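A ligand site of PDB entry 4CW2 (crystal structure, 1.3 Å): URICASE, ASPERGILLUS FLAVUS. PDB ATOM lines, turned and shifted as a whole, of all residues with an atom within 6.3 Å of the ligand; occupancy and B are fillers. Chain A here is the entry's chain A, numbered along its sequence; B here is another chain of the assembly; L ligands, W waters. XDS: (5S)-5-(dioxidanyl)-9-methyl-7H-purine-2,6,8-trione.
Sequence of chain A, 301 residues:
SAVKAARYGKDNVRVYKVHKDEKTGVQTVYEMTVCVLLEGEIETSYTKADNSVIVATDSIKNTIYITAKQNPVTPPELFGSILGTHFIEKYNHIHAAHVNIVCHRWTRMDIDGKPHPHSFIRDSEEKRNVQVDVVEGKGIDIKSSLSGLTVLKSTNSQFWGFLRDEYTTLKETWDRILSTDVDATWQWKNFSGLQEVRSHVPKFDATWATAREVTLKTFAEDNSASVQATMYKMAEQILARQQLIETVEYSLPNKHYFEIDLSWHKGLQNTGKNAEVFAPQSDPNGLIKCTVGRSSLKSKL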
ATOM      1  N   GLN A 158     -21.093  22.345  -9.355  1.00  0.00           N
ATOM      2  CA  GLN A 158     -21.870  23.164  -8.435  1.00  0.00           C
ATOM      3  C   GLN A 158     -22.069  24.542  -9.011  1.00  0.00           C
ATOM      4  O   GLN A 158     -21.297  24.998  -9.873  1.00  0.00           O
ATOM      5  CB  GLN A 158     -21.168  23.260  -7.073  1.00  0.00           C
ATOM      6  CG  GLN A 158     -20.656  21.924  -6.559  1.00  0.00           C
ATOM      7  CD  GLN A 158     -20.098  22.000  -5.183  1.00  0.00           C
ATOM      8  OE1 GLN A 158     -20.562  22.754  -4.320  1.00  0.00           O
ATOM      9  NE2 GLN A 158     -19.091  21.181  -4.944  1.00  0.00           N
ATOM     10  N   PHE A 159     -23.078  25.254  -8.506  1.00  0.00           N
ATOM     11  CA  PHE A 159     -23.222  26.669  -8.836  1.00  0.00           C
ATOM     12  C   PHE A 159     -24.077  27.361  -7.767  1.00  0.00           C
ATOM     13  O   PHE A 159     -25.299  27.278  -7.780  1.00  0.00           O
ATOM     14  CB  PHE A 159     -23.763  26.886 -10.260  1.00  0.00           C
ATOM     15  CG  PHE A 159     -23.644  28.293 -10.743  1.00  0.00           C
ATOM     16  CD1 PHE A 159     -22.380  28.873 -10.897  1.00  0.00           C
ATOM     17  CD2 PHE A 159     -24.732  29.062 -11.031  1.00  0.00           C
ATOM     18  CE1 PHE A 159     -22.257  30.167 -11.326  1.00  0.00           C
ATOM     19  CE2 PHE A 159     -24.635  30.359 -11.486  1.00  0.00           C
ATOM     20  CZ  PHE A 159     -23.381  30.927 -11.621  1.00  0.00           C
ATOM     21  N   LEU A 170     -33.034  31.692 -10.280  1.00  0.00           N
ATOM     22  CA  LEU A 170     -32.262  30.471 -10.228  1.00  0.00           C
ATOM     23  C   LEU A 170     -31.971  29.987  -8.822  1.00  0.00           C
ATOM     24  O   LEU A 170     -31.435  30.758  -8.003  1.00  0.00           O
ATOM     25  CB  LEU A 170     -30.961  30.664 -10.996  1.00  0.00           C
ATOM     26  CG  LEU A 170     -30.002  29.484 -11.100  1.00  0.00           C
ATOM     27  CD1 LEU A 170     -30.602  28.402 -11.989  1.00  0.00           C
ATOM     28  CD2 LEU A 170     -28.666  29.925 -11.690  1.00  0.00           C
ATOM     29  N   ARG A 176     -24.988  19.241  -9.712  1.00  0.00           N
ATOM     30  CA  ARG A 176     -25.657  19.340 -11.016  1.00  0.00           C
ATOM     31  C   ARG A 176     -24.860  18.642 -12.082  1.00  0.00           C
ATOM     32  O   ARG A 176     -23.686  18.277 -11.865  1.00  0.00           O
ATOM     33  CB  ARG A 176     -25.898  20.798 -11.396  1.00  0.00           C
ATOM     34  CG  ARG A 176     -24.621  21.589 -11.668  1.00  0.00           C
ATOM     35  CD  ARG A 176     -24.861  22.959 -12.243  1.00  0.00           C
ATOM     36  NE  ARG A 176     -23.545  23.535 -12.611  1.00  0.00           N
ATOM     37  CZ  ARG A 176     -23.388  24.741 -13.146  1.00  0.00           C
ATOM     38  NH1 ARG A 176     -24.390  25.596 -13.341  1.00  0.00           N
ATOM     39  NH2 ARG A 176     -22.168  25.103 -13.512  1.00  0.00           N
ATOM     40  N   LEU A 178     -22.978  18.978 -15.646  1.00  0.00           N
ATOM     41  CA  LEU A 178     -22.292  19.970 -16.465  1.00  0.00           C
ATOM     42  C   LEU A 178     -21.967  19.339 -17.829  1.00  0.00           C
ATOM     43  O   LEU A 178     -21.301  18.298 -17.864  1.00  0.00           O
ATOM     44  CB  LEU A 178     -21.044  20.497 -15.800  1.00  0.00           C
ATOM     45  CG  LEU A 178     -20.213  21.517 -16.577  1.00  0.00           C
ATOM     46  CD1 LEU A 178     -21.020  22.782 -16.898  1.00  0.00           C
ATOM     47  CD2 LEU A 178     -18.935  21.830 -15.815  1.00  0.00           C
ATOM     48  N   SER A 224     -16.366  21.286  -9.747  1.00  0.00           N
ATOM     49  CA  SER A 224     -16.404  22.618 -10.388  1.00  0.00           C
ATOM     50  C   SER A 224     -17.283  23.626  -9.635  1.00  0.00           C
ATOM     51  O   SER A 224     -18.469  23.368  -9.393  1.00  0.00           O
ATOM     52  CB  SER A 224     -16.955  22.465 -11.795  1.00  0.00           C
ATOM     53  OG  SER A 224     -17.151  23.685 -12.426  1.00  0.00           O
ATOM     54  N   ALA A 225     -16.723  24.789  -9.336  1.00  0.00           N
ATOM     55  CA  ALA A 225     -17.445  25.879  -8.704  1.00  0.00           C
ATOM     56  C   ALA A 225     -18.291  26.663  -9.691  1.00  0.00           C
ATOM     57  O   ALA A 225     -19.228  27.375  -9.330  1.00  0.00           O
ATOM     58  CB  ALA A 225     -16.470  26.814  -8.034  1.00  0.00           C
ATOM     59  N   SER A 226     -17.923  26.564 -10.996  1.00  0.00           N
ATOM     60  CA  SER A 226     -18.538  27.273 -12.097  1.00  0.00           C
ATOM     61  C   SER A 226     -17.782  26.872 -13.370  1.00  0.00           C
ATOM     62  O   SER A 226     -16.636  26.400 -13.291  1.00  0.00           O
ATOM     63  CB  SER A 226     -18.462  28.795 -11.973  1.00  0.00           C
ATOM     64  OG  SER A 226     -17.131  29.262 -12.027  1.00  0.00           O
ATOM     65  N   VAL A 227     -18.408  27.139 -14.513  1.00  0.00           N
ATOM     66  CA  VAL A 227     -17.683  27.002 -15.786  1.00  0.00           C
ATOM     67  C   VAL A 227     -16.439  27.898 -15.792  1.00  0.00           C
ATOM     68  O   VAL A 227     -15.352  27.479 -16.205  1.00  0.00           O
ATOM     69  CB  VAL A 227     -18.621  27.256 -16.963  1.00  0.00           C
ATOM     70  CG1 VAL A 227     -17.855  27.182 -18.292  1.00  0.00           C
ATOM     71  CG2 VAL A 227     -19.784  26.281 -17.004  1.00  0.00           C
ATOM     72  N   GLN A 228     -16.638  29.142 -15.329  1.00  0.00           N
ATOM     73  CA  GLN A 228     -15.560  30.126 -15.268  1.00  0.00           C
ATOM     74  C   GLN A 228     -14.333  29.561 -14.540  1.00  0.00           C
ATOM     75  O   GLN A 228     -13.182  29.669 -15.022  1.00  0.00           O
ATOM     76  CB  GLN A 228     -16.048  31.376 -14.529  1.00  0.00           C
ATOM     77  CG  GLN A 228     -17.036  32.259 -15.241  1.00  0.00           C
ATOM     78  CD  GLN A 228     -18.539  31.874 -15.123  1.00  0.00           C
ATOM     79  OE1 GLN A 228     -18.917  30.724 -14.870  1.00  0.00           O
ATOM     80  NE2 GLN A 228     -19.403  32.853 -15.351  1.00  0.00           N
ATOM     81  N   ASN A 254     -22.829  26.485 -21.737  1.00  0.00           N
ATOM     82  CA  ASN A 254     -23.381  25.704 -20.621  1.00  0.00           C
ATOM     83  C   ASN A 254     -24.677  25.087 -21.080  1.00  0.00           C
ATOM     84  O   ASN A 254     -25.674  25.787 -21.259  1.00  0.00           O
ATOM     85  CB  ASN A 254     -23.571  26.600 -19.395  1.00  0.00           C
ATOM     86  CG  ASN A 254     -23.835  25.805 -18.138  1.00  0.00           C
ATOM     87  OD1 ASN A 254     -23.835  24.568 -18.135  1.00  0.00           O
ATOM     88  ND2 ASN A 254     -24.041  26.525 -17.033  1.00  0.00           N
ATOM     89  N   HIS A 256     -27.656  23.214 -20.660  1.00  0.00           N
ATOM     90  CA  HIS A 256     -28.378  22.959 -19.419  1.00  0.00           C
ATOM     91  C   HIS A 256     -29.183  21.673 -19.489  1.00  0.00           C
ATOM     92  O   HIS A 256     -29.814  21.345 -20.498  1.00  0.00           O
ATOM     93  CB  HIS A 256     -29.308  24.129 -19.101  1.00  0.00           C
ATOM     94  CG  HIS A 256     -28.629  25.465 -19.074  1.00  0.00           C
ATOM     95  ND1 HIS A 256     -27.695  25.814 -18.118  1.00  0.00           N
ATOM     96  CD2 HIS A 256     -28.732  26.520 -19.894  1.00  0.00           C
ATOM     97  CE1 HIS A 256     -27.248  27.033 -18.388  1.00  0.00           C
ATOM     98  NE2 HIS A 256     -27.852  27.488 -19.467  1.00  0.00           N
ATOM     99  N   ASN A 285     -28.761  28.791 -23.876  1.00  0.00           N
ATOM    100  CA  ASN A 285     -27.599  28.245 -23.210  1.00  0.00           C
ATOM    101  C   ASN A 285     -26.707  29.349 -22.694  1.00  0.00           C
ATOM    102  O   ASN A 285     -26.502  30.365 -23.347  1.00  0.00           O
ATOM    103  CB  ASN A 285     -26.748  27.325 -24.132  1.00  0.00           C
ATOM    104  CG  ASN A 285     -26.253  28.007 -25.380  1.00  0.00           C
ATOM    105  OD1 ASN A 285     -26.983  28.130 -26.340  1.00  0.00           O
ATOM    106  ND2 ASN A 285     -24.997  28.412 -25.374  1.00  0.00           N
ATOM    107  N   GLY A 286     -26.139  29.126 -21.497  1.00  0.00           N
ATOM    108  CA  GLY A 286     -25.062  30.011 -21.063  1.00  0.00           C
ATOM    109  C   GLY A 286     -23.933  29.933 -22.095  1.00  0.00           C
ATOM    110  O   GLY A 286     -23.730  28.895 -22.760  1.00  0.00           O
ATOM    111  N   LEU A 287     -23.135  31.004 -22.169  1.00  0.00           N
ATOM    112  CA  LEU A 287     -21.950  31.039 -23.025  1.00  0.00           C
ATOM    113  C   LEU A 287     -20.879  31.825 -22.256  1.00  0.00           C
ATOM    114  O   LEU A 287     -21.105  32.999 -21.879  1.00  0.00           O
ATOM    115  CB  LEU A 287     -22.249  31.712 -24.371  1.00  0.00           C
ATOM    116  CG  LEU A 287     -21.085  31.889 -25.330  1.00  0.00           C
ATOM    117  CD1 LEU A 287     -20.429  30.514 -25.632  1.00  0.00           C
ATOM    118  CD2 LEU A 287     -21.529  32.570 -26.619  1.00  0.00           C
ATOM    119  N   ILE A 288     -19.800  31.115 -21.959  1.00  0.00           N
ATOM    120  CA  ILE A 288     -18.790  31.619 -21.018  1.00  0.00           C
ATOM    121  C   ILE A 288     -17.456  31.639 -21.789  1.00  0.00           C
ATOM    122  O   ILE A 288     -17.048  30.639 -22.391  1.00  0.00           O
ATOM    123  CB  ILE A 288     -18.646  30.685 -19.789  1.00  0.00           C
ATOM    124  CG1 ILE A 288     -20.026  30.182 -19.272  1.00  0.00           C
ATOM    125  CG2 ILE A 288     -17.862  31.382 -18.704  1.00  0.00           C
ATOM    126  CD1 ILE A 288     -20.960  31.273 -18.771  1.00  0.00           C
ATOM    127  N   TYR B   8     -19.292  36.857 -20.675  1.00  0.00           N
ATOM    128  CA  TYR B   8     -20.146  35.700 -20.469  1.00  0.00           C
ATOM    129  C   TYR B   8     -21.607  36.149 -20.454  1.00  0.00           C
ATOM    130  O   TYR B   8     -21.927  37.313 -20.186  1.00  0.00           O
ATOM    131  CB  TYR B   8     -19.782  34.985 -19.115  1.00  0.00           C
ATOM    132  CG  TYR B   8     -20.476  35.663 -17.954  1.00  0.00           C
ATOM    133  CD1 TYR B   8     -20.031  36.914 -17.502  1.00  0.00           C
ATOM    134  CD2 TYR B   8     -21.644  35.150 -17.409  1.00  0.00           C
ATOM    135  CE1 TYR B   8     -20.773  37.635 -16.570  1.00  0.00           C
ATOM    136  CE2 TYR B   8     -22.352  35.843 -16.477  1.00  0.00           C
ATOM    137  CZ  TYR B   8     -21.934  37.088 -16.062  1.00  0.00           C
ATOM    138  OH  TYR B   8     -22.663  37.824 -15.172  1.00  0.00           O
ATOM    139  N   GLY B   9     -22.505  35.217 -20.735  1.00  0.00           N
ATOM    140  CA  GLY B   9     -23.919  35.584 -20.705  1.00  0.00           C
ATOM    141  C   GLY B   9     -24.786  34.473 -21.264  1.00  0.00           C
ATOM    142  O   GLY B   9     -24.418  33.297 -21.191  1.00  0.00           O
ATOM    143  N   LYS B  10     -25.973  34.881 -21.760  1.00  0.00           N
ATOM    144  CA  LYS B  10     -26.916  33.889 -22.288  1.00  0.00           C
ATOM    145  C   LYS B  10     -27.043  34.072 -23.798  1.00  0.00           C
ATOM    146  O   LYS B  10     -27.283  35.177 -24.286  1.00  0.00           O
ATOM    147  CB  LYS B  10     -28.327  33.976 -21.659  1.00  0.00           C
ATOM    148  CG  LYS B  10     -29.146  32.719 -21.914  1.00  0.00           C
ATOM    149  CD  LYS B  10     -28.716  31.492 -21.105  1.00  0.00           C
ATOM    150  CE  LYS B  10     -29.467  31.301 -19.820  1.00  0.00           C
ATOM    151  NZ  LYS B  10     -28.765  30.391 -18.906  1.00  0.00           N
ATOM    152  N   ASN B  51     -18.219  33.595  -7.087  1.00  0.00           N
ATOM    153  CA  ASN B  51     -19.439  33.740  -7.851  1.00  0.00           C
ATOM    154  C   ASN B  51     -20.241  34.994  -7.543  1.00  0.00           C
ATOM    155  O   ASN B  51     -21.175  35.331  -8.222  1.00  0.00           O
ATOM    156  CB  ASN B  51     -20.323  32.494  -7.752  1.00  0.00           C
ATOM    157  CG  ASN B  51     -19.727  31.311  -8.521  1.00  0.00           C
ATOM    158  OD1 ASN B  51     -18.961  31.504  -9.509  1.00  0.00           O
ATOM    159  ND2 ASN B  51     -20.065  30.116  -8.101  1.00  0.00           N
ATOM    160  N   ILE B  54     -20.956  37.313 -10.367  1.00  0.00           N
ATOM    161  CA  ILE B  54     -21.705  36.806 -11.519  1.00  0.00           C
ATOM    162  C   ILE B  54     -23.175  37.099 -11.405  1.00  0.00           C
ATOM    163  O   ILE B  54     -23.861  36.623 -10.491  1.00  0.00           O
ATOM    164  CB  ILE B  54     -21.476  35.300 -11.729  1.00  0.00           C
ATOM    165  CG1 ILE B  54     -20.006  35.046 -12.056  1.00  0.00           C
ATOM    166  CG2 ILE B  54     -22.388  34.793 -12.833  1.00  0.00           C
ATOM    167  CD1 ILE B  54     -19.487  35.855 -13.219  1.00  0.00           C
ATOM    168  N   VAL B  55     -23.655  37.904 -12.352  1.00  0.00           N
ATOM    169  CA  VAL B  55     -25.073  37.986 -12.685  1.00  0.00           C
ATOM    170  C   VAL B  55     -25.403  36.742 -13.467  1.00  0.00           C
ATOM    171  O   VAL B  55     -24.869  36.524 -14.569  1.00  0.00           O
ATOM    172  CB  VAL B  55     -25.403  39.263 -13.493  1.00  0.00           C
ATOM    173  CG1 VAL B  55     -26.867  39.303 -13.868  1.00  0.00           C
ATOM    174  CG2 VAL B  55     -24.992  40.535 -12.716  1.00  0.00           C
ATOM    175  N   ALA B  56     -26.161  35.819 -12.896  1.00  0.00           N
ATOM    176  CA  ALA B  56     -26.294  34.481 -13.506  1.00  0.00           C
ATOM    177  C   ALA B  56     -26.850  34.636 -14.906  1.00  0.00           C
ATOM    178  O   ALA B  56     -27.694  35.484 -15.196  1.00  0.00           O
ATOM    179  CB  ALA B  56     -27.261  33.634 -12.670  1.00  0.00           C
ATOM    180  N   THR B  57     -26.358  33.754 -15.814  1.00  0.00           N
ATOM    181  CA  THR B  57     -26.912  33.788 -17.170  1.00  0.00           C
ATOM    182  C   THR B  57     -28.437  33.535 -17.166  1.00  0.00           C
ATOM    183  O   THR B  57     -29.172  34.119 -17.967  1.00  0.00           O
ATOM    184  CB  THR B  57     -26.179  32.837 -18.153  1.00  0.00           C
ATOM    185  OG1 THR B  57     -26.497  31.466 -17.902  1.00  0.00           O
ATOM    186  CG2 THR B  57     -24.681  33.074 -18.077  1.00  0.00           C
ATOM    187  N   ASP B  58     -28.902  32.716 -16.203  1.00  0.00           N
ATOM    188  CA  ASP B  58     -30.354  32.511 -16.072  1.00  0.00           C
ATOM    189  C   ASP B  58     -31.083  33.847 -15.794  1.00  0.00           C
ATOM    190  O   ASP B  58     -32.180  34.095 -16.308  1.00  0.00           O
ATOM    191  CB  ASP B  58     -30.629  31.525 -14.943  1.00  0.00           C
ATOM    192  CG  ASP B  58     -32.054  31.099 -14.901  1.00  0.00           C
ATOM    193  OD1 ASP B  58     -32.428  30.208 -15.716  1.00  0.00           O
ATOM    194  OD2 ASP B  58     -32.841  31.657 -14.098  1.00  0.00           O
ATOM    195  N   SER B  59     -30.455  34.708 -14.948  1.00  0.00           N
ATOM    196  CA  SER B  59     -30.993  36.036 -14.677  1.00  0.00           C
ATOM    197  C   SER B  59     -30.943  36.966 -15.890  1.00  0.00           C
ATOM    198  O   SER B  59     -31.834  37.780 -16.074  1.00  0.00           O
ATOM    199  CB  SER B  59     -30.274  36.678 -13.493  1.00  0.00           C
ATOM    200  OG  SER B  59     -30.328  35.805 -12.326  1.00  0.00           O
HETATM  201  O4  XDS L   1     -21.241  27.792 -14.269  1.00  0.00           O
HETATM  202  C4  XDS L   1     -22.115  28.620 -14.457  1.00  0.00           C
HETATM  203  N2  XDS L   1     -21.759  29.962 -14.670  1.00  0.00           N
HETATM  204  C3  XDS L   1     -22.595  30.994 -14.973  1.00  0.00           C
HETATM  205  O3  XDS L   1     -22.250  32.170 -15.051  1.00  0.00           O
HETATM  206  N3  XDS L   1     -23.463  28.260 -14.360  1.00  0.00           N
HETATM  207  C5  XDS L   1     -24.304  29.168 -14.681  1.00  0.00           C
HETATM  208  N   XDS L   1     -25.653  29.222 -14.543  1.00  0.00           N
HETATM  209  C   XDS L   1     -26.487  28.085 -14.155  1.00  0.00           C
HETATM  210  C2  XDS L   1     -24.005  30.529 -15.322  1.00  0.00           C
HETATM  211  O1  XDS L   1     -23.667  30.188 -16.757  1.00  0.00           O
HETATM  212  O2  XDS L   1     -24.765  29.498 -17.464  1.00  0.00           O
HETATM  213  N1  XDS L   1     -25.134  31.371 -15.135  1.00  0.00           N
HETATM  214  C1  XDS L   1     -26.150  30.505 -14.797  1.00  0.00           C
HETATM  215  O   XDS L   1     -27.343  30.818 -14.704  1.00  0.00           O
HETATM  216  O   HOH W   1     -27.206  25.559 -12.149  1.00  0.00           O
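N of Gly 286 is in hydrogen-bond range of NE2 of His 256, at 3.1 Å. The side-chain hydroxyl (OH) of Tyr 8 of chain B lies within hydrogen-bond range of the backbone carbonyl oxygen (O) of Val 55 of chain B. O of Ser 226 lies within hydrogen-bond range of OG of Ser 224 (2.9 Å). N of Gln 228 lies close to OG of Ser 226 (3.3 Å). The backbone NH (N) of Asn 254 is in hydrogen-bond range of the backbone carbonyl oxygen (O) of Gly 286, 2.8 Å away. A ring nitrogen (NE2) of His 256 is in hydrogen-bond range of the side-chain amino group of Lys 10 of chain B, at 3.1 Å. A ring nitrogen (NE2) of His 256 is in hydrogen-bond range of the backbone carbonyl oxygen of Asn 254 (3.3 Å). OG1 of Thr 57 of chain B is in hydrogen-bond range of NZ of Lys 10 of chain B, at 2.7 Å.
ND2 of Asn 254 is in hydrogen-bond range of O2 of the ligand (3.1 Å). NE2 of Gln 228 is in hydrogen-bond range of O3 of the ligand, at 2.9 Å. O of the ligand is in hydrogen-bond range of N of Asp 58 of chain B. The side-chain hydroxyl (OG1) of Thr 57 of chain B sits at hydrogen-bond distance from an oxygen (O2) of the ligand, at 2.7 Å. The guanidinium group (NH2) of Arg 176 is in hydrogen-bond range of an oxygen (O4) of the ligand, at 2.9 Å. N of Thr 57 of chain B sits at hydrogen-bond distance from O of the ligand. The backbone NH of Val 227 lies within hydrogen-bond range of an oxygen (O4) of the ligand (2.9 Å).
Merely in contact with the ligand: Phe 159 (3.4 Å), Leu 170 (3.4 Å), Ser 226 (3.5 Å), His 256 (3.6 Å), Gly 286 (3.6 Å), Ile 288 (3.5 Å), Tyr 8 of chain B (3.8 Å), Ile 54 of chain B (3.4 Å) and Ala 56 of chain B (3.5 Å). Hydrophobic or aromatic side chains that line the ligand: Phe 159, Leu 170, Val 227, His 256, Ile 288, Tyr 8 of chain B, Ile 54 of chain B and Ala 56 of chain B.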
